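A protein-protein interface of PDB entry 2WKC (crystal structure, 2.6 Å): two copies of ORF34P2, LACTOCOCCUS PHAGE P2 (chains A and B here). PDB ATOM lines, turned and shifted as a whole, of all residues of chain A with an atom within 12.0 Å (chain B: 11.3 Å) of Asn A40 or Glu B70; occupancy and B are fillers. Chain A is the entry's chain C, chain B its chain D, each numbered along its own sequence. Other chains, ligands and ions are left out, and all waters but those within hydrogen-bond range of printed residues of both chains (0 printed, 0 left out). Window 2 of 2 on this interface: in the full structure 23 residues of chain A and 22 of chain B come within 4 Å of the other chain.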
ATOM      1  N   PHE A  33      19.834  11.185 -11.480  1.00  0.00           N
ATOM      2  CA  PHE A  33      20.615   9.998 -11.825  1.00  0.00           C
ATOM      3  C   PHE A  33      21.908  10.002 -11.045  1.00  0.00           C
ATOM      4  O   PHE A  33      22.162  10.918 -10.279  1.00  0.00           O
ATOM      5  CB  PHE A  33      20.863   9.856 -13.340  1.00  0.00           C
ATOM      6  CG  PHE A  33      21.041  11.160 -14.065  1.00  0.00           C
ATOM      7  CD1 PHE A  33      22.280  11.781 -14.111  1.00  0.00           C
ATOM      8  CD2 PHE A  33      19.967  11.752 -14.726  1.00  0.00           C
ATOM      9  CE1 PHE A  33      22.447  12.993 -14.789  1.00  0.00           C
ATOM     10  CE2 PHE A  33      20.121  12.952 -15.401  1.00  0.00           C
ATOM     11  CZ  PHE A  33      21.367  13.577 -15.433  1.00  0.00           C
ATOM     12  N   GLU A  34      22.720   8.971 -11.241  1.00  0.00           N
ATOM     13  CA  GLU A  34      23.923   8.773 -10.444  1.00  0.00           C
ATOM     14  C   GLU A  34      25.201   9.038 -11.243  1.00  0.00           C
ATOM     15  O   GLU A  34      25.189   9.059 -12.472  1.00  0.00           O
ATOM     16  CB  GLU A  34      23.920   7.365  -9.829  1.00  0.00           C
ATOM     17  CG  GLU A  34      22.748   7.153  -8.875  1.00  0.00           C
ATOM     18  CD  GLU A  34      22.591   5.717  -8.407  1.00  0.00           C
ATOM     19  OE1 GLU A  34      23.338   4.835  -8.892  1.00  0.00           O
ATOM     20  OE2 GLU A  34      21.708   5.481  -7.547  1.00  0.00           O
ATOM     21  N   LYS A  35      26.293   9.253 -10.521  1.00  0.00           N
ATOM     22  CA  LYS A  35      27.564   9.623 -11.118  1.00  0.00           C
ATOM     23  C   LYS A  35      28.684   8.916 -10.374  1.00  0.00           C
ATOM     24  O   LYS A  35      28.482   8.423  -9.264  1.00  0.00           O
ATOM     25  CB  LYS A  35      27.766  11.145 -11.053  1.00  0.00           C
ATOM     26  CG  LYS A  35      27.842  11.716  -9.632  1.00  0.00           C
ATOM     27  CD  LYS A  35      28.035  13.220  -9.627  1.00  0.00           C
ATOM     28  CE  LYS A  35      29.476  13.602  -9.883  1.00  0.00           C
ATOM     29  NZ  LYS A  35      29.597  15.056 -10.140  1.00  0.00           N
ATOM     30  N   GLU A  36      29.854   8.853 -10.995  1.00  0.00           N
ATOM     31  CA  GLU A  36      31.056   8.406 -10.311  1.00  0.00           C
ATOM     32  C   GLU A  36      31.425   9.491  -9.303  1.00  0.00           C
ATOM     33  O   GLU A  36      31.578  10.658  -9.669  1.00  0.00           O
ATOM     34  CB  GLU A  36      32.191   8.158 -11.314  1.00  0.00           C
ATOM     35  CG  GLU A  36      31.888   7.061 -12.348  1.00  0.00           C
ATOM     36  CD  GLU A  36      32.830   7.060 -13.557  1.00  0.00           C
ATOM     37  OE1 GLU A  36      33.349   8.131 -13.944  1.00  0.00           O
ATOM     38  OE2 GLU A  36      33.041   5.972 -14.138  1.00  0.00           O
ATOM     39  N   LYS A  37      31.512   9.114  -8.031  1.00  0.00           N
ATOM     40  CA  LYS A  37      31.972  10.023  -6.975  1.00  0.00           C
ATOM     41  C   LYS A  37      33.340  10.608  -7.348  1.00  0.00           C
ATOM     42  O   LYS A  37      34.256   9.872  -7.734  1.00  0.00           O
ATOM     43  CB  LYS A  37      32.046   9.291  -5.628  1.00  0.00           C
ATOM     44  CG  LYS A  37      30.860   8.363  -5.372  1.00  0.00           C
ATOM     45  CD  LYS A  37      30.625   8.093  -3.892  1.00  0.00           C
ATOM     46  CE  LYS A  37      29.198   7.587  -3.667  1.00  0.00           C
ATOM     47  NZ  LYS A  37      28.694   7.856  -2.285  1.00  0.00           N
ATOM     48  N   GLY A  38      33.458  11.930  -7.268  1.00  0.00           N
ATOM     49  CA  GLY A  38      34.681  12.625  -7.672  1.00  0.00           C
ATOM     50  C   GLY A  38      34.824  12.779  -9.179  1.00  0.00           C
ATOM     51  O   GLY A  38      35.899  13.108  -9.682  1.00  0.00           O
ATOM     52  N   SER A  39      33.732  12.539  -9.899  1.00  0.00           N
ATOM     53  CA  SER A  39      33.685  12.723 -11.348  1.00  0.00           C
ATOM     54  C   SER A  39      33.231  14.136 -11.726  1.00  0.00           C
ATOM     55  O   SER A  39      32.500  14.795 -10.974  1.00  0.00           O
ATOM     56  CB  SER A  39      32.778  11.659 -11.978  1.00  0.00           C
ATOM     57  OG  SER A  39      31.842  12.207 -12.888  1.00  0.00           O
ATOM     58  N   ASN A  40      33.657  14.568 -12.910  1.00  0.00           N
ATOM     59  CA  ASN A  40      33.395  15.917 -13.420  1.00  0.00           C
ATOM     60  C   ASN A  40      32.000  16.172 -14.045  1.00  0.00           C
ATOM     61  O   ASN A  40      31.696  17.311 -14.418  1.00  0.00           O
ATOM     62  CB  ASN A  40      34.492  16.288 -14.423  1.00  0.00           C
ATOM     63  CG  ASN A  40      34.893  17.749 -14.344  1.00  0.00           C
ATOM     64  OD1 ASN A  40      34.044  18.643 -14.308  1.00  0.00           O
ATOM     65  ND2 ASN A  40      36.196  17.999 -14.323  1.00  0.00           N
ATOM     66  N   VAL A  41      31.159  15.138 -14.147  1.00  0.00           N
ATOM     67  CA  VAL A  41      29.852  15.261 -14.822  1.00  0.00           C
ATOM     68  C   VAL A  41      28.758  15.900 -13.954  1.00  0.00           C
ATOM     69  O   VAL A  41      28.819  15.862 -12.720  1.00  0.00           O
ATOM     70  CB  VAL A  41      29.326  13.909 -15.436  1.00  0.00           C
ATOM     71  CG1 VAL A  41      30.360  13.275 -16.357  1.00  0.00           C
ATOM     72  CG2 VAL A  41      28.877  12.925 -14.359  1.00  0.00           C
ATOM     73  N   LYS A  42      27.751  16.458 -14.626  1.00  0.00           N
ATOM     74  CA  LYS A  42      26.707  17.249 -13.995  1.00  0.00           C
ATOM     75  C   LYS A  42      25.422  16.456 -13.841  1.00  0.00           C
ATOM     76  O   LYS A  42      24.906  15.885 -14.803  1.00  0.00           O
ATOM     77  CB  LYS A  42      26.447  18.517 -14.804  1.00  0.00           C
ATOM     78  CG  LYS A  42      27.613  19.505 -14.802  1.00  0.00           C
ATOM     79  CD  LYS A  42      27.815  20.155 -13.435  1.00  0.00           C
ATOM     80  CE  LYS A  42      29.200  20.771 -13.320  1.00  0.00           C
ATOM     81  NZ  LYS A  42      29.524  21.194 -11.925  1.00  0.00           N
ATOM     82  N   VAL A  43      24.906  16.424 -12.620  1.00  0.00           N
ATOM     83  CA  VAL A  43      23.686  15.704 -12.340  1.00  0.00           C
ATOM     84  C   VAL A  43      22.540  16.703 -12.251  1.00  0.00           C
ATOM     85  O   VAL A  43      22.625  17.694 -11.533  1.00  0.00           O
ATOM     86  CB  VAL A  43      23.814  14.862 -11.032  1.00  0.00           C
ATOM     87  CG1 VAL A  43      22.481  14.269 -10.630  1.00  0.00           C
ATOM     88  CG2 VAL A  43      24.846  13.762 -11.201  1.00  0.00           C
ATOM     89  N   ALA A  44      21.475  16.443 -13.000  1.00  0.00           N
ATOM     90  CA  ALA A  44      20.265  17.243 -12.913  1.00  0.00           C
ATOM     91  C   ALA A  44      19.499  16.946 -11.618  1.00  0.00           C
ATOM     92  O   ALA A  44      19.295  15.782 -11.245  1.00  0.00           O
ATOM     93  CB  ALA A  44      19.382  16.992 -14.135  1.00  0.00           C
ATOM     94  N   TYR A  45      19.077  18.000 -10.934  1.00  0.00           N
ATOM     95  CA  TYR A  45      18.277  17.847  -9.717  1.00  0.00           C
ATOM     96  C   TYR A  45      16.814  18.228  -9.928  1.00  0.00           C
ATOM     97  O   TYR A  45      16.508  19.200 -10.627  1.00  0.00           O
ATOM     98  CB  TYR A  45      18.881  18.661  -8.574  1.00  0.00           C
ATOM     99  CG  TYR A  45      20.006  17.960  -7.862  1.00  0.00           C
ATOM    100  CD1 TYR A  45      19.881  17.588  -6.528  1.00  0.00           C
ATOM    101  CD2 TYR A  45      21.192  17.654  -8.521  1.00  0.00           C
ATOM    102  CE1 TYR A  45      20.908  16.947  -5.864  1.00  0.00           C
ATOM    103  CE2 TYR A  45      22.221  17.006  -7.869  1.00  0.00           C
ATOM    104  CZ  TYR A  45      22.076  16.659  -6.536  1.00  0.00           C
ATOM    105  OH  TYR A  45      23.102  16.009  -5.884  1.00  0.00           O
ATOM    106  N   VAL B  66      20.574   4.448 -13.209  1.00  0.00           N
ATOM    107  CA  VAL B  66      21.214   5.080 -14.349  1.00  0.00           C
ATOM    108  C   VAL B  66      22.439   5.832 -13.864  1.00  0.00           C
ATOM    109  O   VAL B  66      22.351   6.680 -12.964  1.00  0.00           O
ATOM    110  CB  VAL B  66      20.264   6.011 -15.096  1.00  0.00           C
ATOM    111  CG1 VAL B  66      21.010   6.765 -16.198  1.00  0.00           C
ATOM    112  CG2 VAL B  66      19.102   5.213 -15.683  1.00  0.00           C
ATOM    113  N   GLN B  67      23.584   5.490 -14.444  1.00  0.00           N
ATOM    114  CA  GLN B  67      24.831   6.158 -14.129  1.00  0.00           C
ATOM    115  C   GLN B  67      25.294   7.003 -15.322  1.00  0.00           C
ATOM    116  O   GLN B  67      25.257   6.550 -16.468  1.00  0.00           O
ATOM    117  CB  GLN B  67      25.901   5.137 -13.704  1.00  0.00           C
ATOM    118  CG  GLN B  67      27.135   5.770 -13.063  1.00  0.00           C
ATOM    119  CD  GLN B  67      27.968   4.790 -12.248  1.00  0.00           C
ATOM    120  OE1 GLN B  67      28.600   3.885 -12.794  1.00  0.00           O
ATOM    121  NE2 GLN B  67      27.987   4.983 -10.931  1.00  0.00           N
ATOM    122  N   ALA B  68      25.710   8.235 -15.044  1.00  0.00           N
ATOM    123  CA  ALA B  68      26.312   9.102 -16.050  1.00  0.00           C
ATOM    124  C   ALA B  68      27.837   8.966 -16.015  1.00  0.00           C
ATOM    125  O   ALA B  68      28.466   9.287 -15.004  1.00  0.00           O
ATOM    126  CB  ALA B  68      25.892  10.542 -15.823  1.00  0.00           C
ATOM    127  N   LYS B  69      28.421   8.485 -17.116  1.00  0.00           N
ATOM    128  CA  LYS B  69      29.865   8.209 -17.190  1.00  0.00           C
ATOM    129  C   LYS B  69      30.647   9.216 -18.025  1.00  0.00           C
ATOM    130  O   LYS B  69      30.164   9.686 -19.056  1.00  0.00           O
ATOM    131  CB  LYS B  69      30.130   6.804 -17.742  1.00  0.00           C
ATOM    132  CG  LYS B  69      30.095   5.696 -16.697  1.00  0.00           C
ATOM    133  CD  LYS B  69      30.625   4.375 -17.255  1.00  0.00           C
ATOM    134  CE  LYS B  69      32.153   4.350 -17.317  1.00  0.00           C
ATOM    135  NZ  LYS B  69      32.662   3.026 -17.761  1.00  0.00           N
ATOM    136  N   GLU B  70      31.865   9.519 -17.572  1.00  0.00           N
ATOM    137  CA  GLU B  70      32.767  10.424 -18.268  1.00  0.00           C
ATOM    138  C   GLU B  70      33.648   9.637 -19.229  1.00  0.00           C
ATOM    139  O   GLU B  70      33.172   9.136 -20.245  1.00  0.00           O
ATOM    140  CB  GLU B  70      33.622  11.208 -17.268  1.00  0.00           C
ATOM    141  CG  GLU B  70      34.337  12.443 -17.851  1.00  0.00           C
ATOM    142  CD  GLU B  70      35.166  13.200 -16.819  1.00  0.00           C
ATOM    143  OE1 GLU B  70      34.834  13.139 -15.613  1.00  0.00           O
ATOM    144  OE2 GLU B  70      36.150  13.864 -17.214  1.00  0.00           O
ATOM    145  N   TYR B  74      33.132  14.023 -21.866  1.00  0.00           N
ATOM    146  CA  TYR B  74      31.882  13.534 -22.448  1.00  0.00           C
ATOM    147  C   TYR B  74      31.085  12.630 -21.519  1.00  0.00           C
ATOM    148  O   TYR B  74      31.661  11.841 -20.769  1.00  0.00           O
ATOM    149  CB  TYR B  74      32.141  12.829 -23.778  1.00  0.00           C
ATOM    150  CG  TYR B  74      31.964  13.747 -24.959  1.00  0.00           C
ATOM    151  CD1 TYR B  74      30.734  13.835 -25.613  1.00  0.00           C
ATOM    152  CD2 TYR B  74      33.011  14.547 -25.407  1.00  0.00           C
ATOM    153  CE1 TYR B  74      30.558  14.686 -26.694  1.00  0.00           C
ATOM    154  CE2 TYR B  74      32.845  15.401 -26.486  1.00  0.00           C
ATOM    155  CZ  TYR B  74      31.615  15.466 -27.125  1.00  0.00           C
ATOM    156  OH  TYR B  74      31.443  16.308 -28.198  1.00  0.00           O
ATOM    157  N   VAL B  75      29.758  12.752 -21.596  1.00  0.00           N
ATOM    158  CA  VAL B  75      28.828  12.044 -20.714  1.00  0.00           C
ATOM    159  C   VAL B  75      27.892  11.095 -21.479  1.00  0.00           C
ATOM    160  O   VAL B  75      27.312  11.468 -22.505  1.00  0.00           O
ATOM    161  CB  VAL B  75      27.991  13.041 -19.832  1.00  0.00           C
ATOM    162  CG1 VAL B  75      27.126  13.976 -20.694  1.00  0.00           C
ATOM    163  CG2 VAL B  75      27.125  12.300 -18.807  1.00  0.00           C
ATOM    164  N   ASN B  76      27.767   9.868 -20.974  1.00  0.00           N
ATOM    165  CA  ASN B  76      26.763   8.919 -21.449  1.00  0.00           C
ATOM    166  C   ASN B  76      25.933   8.417 -20.283  1.00  0.00           C
ATOM    167  O   ASN B  76      26.469   8.141 -19.205  1.00  0.00           O
ATOM    168  CB  ASN B  76      27.405   7.727 -22.177  1.00  0.00           C
ATOM    169  CG  ASN B  76      27.465   7.911 -23.697  1.00  0.00           C
ATOM    170  OD1 ASN B  76      28.528   7.783 -24.301  1.00  0.00           O
ATOM    171  ND2 ASN B  76      26.318   8.198 -24.316  1.00  0.00           N
ATOM    172  N   TYR B  77      24.628   8.307 -20.506  1.00  0.00           N
ATOM    173  CA  TYR B  77      23.711   7.818 -19.493  1.00  0.00           C
ATOM    174  C   TYR B  77      23.400   6.355 -19.758  1.00  0.00           C
ATOM    175  O   TYR B  77      22.710   6.017 -20.723  1.00  0.00           O
ATOM    176  CB  TYR B  77      22.433   8.642 -19.489  1.00  0.00           C
ATOM    177  CG  TYR B  77      22.662  10.130 -19.404  1.00  0.00           C
ATOM    178  CD1 TYR B  77      22.886  10.752 -18.172  1.00  0.00           C
ATOM    179  CD2 TYR B  77      22.649  10.922 -20.558  1.00  0.00           C
ATOM    180  CE1 TYR B  77      23.086  12.122 -18.093  1.00  0.00           C
ATOM    181  CE2 TYR B  77      22.852  12.286 -20.490  1.00  0.00           C
ATOM    182  CZ  TYR B  77      23.067  12.884 -19.255  1.00  0.00           C
ATOM    183  OH  TYR B  77      23.279  14.243 -19.186  1.00  0.00           O
ATOM    184  N   ASN B  78      23.923   5.493 -18.893  1.00  0.00           N
ATOM    185  CA  ASN B  78      23.839   4.052 -19.075  1.00  0.00           C
ATOM    186  C   ASN B  78      23.096   3.391 -17.938  1.00  0.00           C
ATOM    187  O   ASN B  78      23.295   3.731 -16.777  1.00  0.00           O
ATOM    188  CB  ASN B  78      25.240   3.442 -19.196  1.00  0.00           C
ATOM    189  CG  ASN B  78      25.989   3.928 -20.422  1.00  0.00           C
ATOM    190  OD1 ASN B  78      25.411   4.082 -21.499  1.00  0.00           O
ATOM    191  ND2 ASN B  78      27.289   4.164 -20.266  1.00  0.00           N
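No position is printed for both chains.
The backbone NH of Glu A34 is in hydrogen-bond range of the backbone carbonyl oxygen of Val B66 (2.9 Å). The backbone NH of Ala B68 lies within hydrogen-bond range of the backbone carbonyl oxygen of Glu A34, 2.8 Å away. N of Asn A40 is in hydrogen-bond range of OE1 of Glu B70 (3.3 Å).
Phe A33 touches Val B66 (CB to O, 3.5 Å). Phe A33 touches Tyr B77. Gln B67 touches Glu A34. Lys A35 touches Gln B67 (O to NE2, 3.9 Å). Glu A36 touches Lys B69 (OE2 to CE, 3.7 Å). CG2 of Val A41 touches O of Ala B68 (3.7 Å). Val A41 touches Glu B70 (CG1 to CB, 3.97 Å).
O of Ser A39 is in hydrogen-bond range of NZ of Lys A35. The side-chain amino group (NZ) of Lys A35 sits at hydrogen-bond distance from the backbone carbonyl oxygen (O) of Val A41 (2.8 Å). N of Val A41 sits at hydrogen-bond distance from OG of Ser A39 (3.3 Å). N of Gln B67 sits at hydrogen-bond distance from O of Asn B78 (2.9 Å). The backbone carbonyl oxygen (O) of Asn B76 lies within hydrogen-bond range of the backbone NH (N) of Lys B69 (2.9 Å).
Printed residues of chain A that touch a printed residue of chain B: Phe A33, Glu A34, Lys A35, Glu A36, Asn A40 and Val A41. Hydrophobic or aromatic side chains of chain A that line the printed part of chain B: Phe A33 and Val A41. Along chain A the printed residues that touch a printed residue of chain B span positions 33 to 41. Of the 10 printed residues of chain B, 6 touch a printed residue of chain A. Printed residues of chain B that touch a printed residue of chain A: Val B66, Gln B67, Ala B68, Lys B69, Glu B70 and Tyr B77.
Glu B70 touches just these residues of chain A: Asn A40 and Val A41. Glu A36 touches one residue of chain B. No residue of chain B comes within 4 Å of Gly A38. Of chain B, only Ala B68 and Glu B70 come within 4 Å of Val A41. No residue of chain B comes within 4 Å of Lys A42. Of chain A, only Glu A36 (3.7 Å) comes within 4 Å of Lys B69. Val B75 touches none of the printed residues of chain A. Of the printed residues of chain B, Glu A34 touches Val B66 (2.9 Å), Gln B67 (3.4 Å) and Ala B68 (2.8 Å). Of the printed residues of chain A, Ala B68 touches Glu A34 and Val A41. Of the printed residues of chain A, Gln B67 touches Glu A34 and Lys A35. Of the printed residues of chain B, Phe A33 touches Val B66 and Tyr B77. Of the printed residues of chain A, Val B66 touches Phe A33 (3.5 Å) and Glu A34 (2.9 Å). Asn B76 touches none of the printed residues of chain A. The nearest printed residue of chain B that does not touch Asn A40 is Ala B68 (7.7 Å). The nearest printed residue of chain A that does not touch Glu B70 is Ser A39 (4.2 Å). The nearest printed residue of chain A that does not touch Tyr B77 is Lys A42 (5.0 Å).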
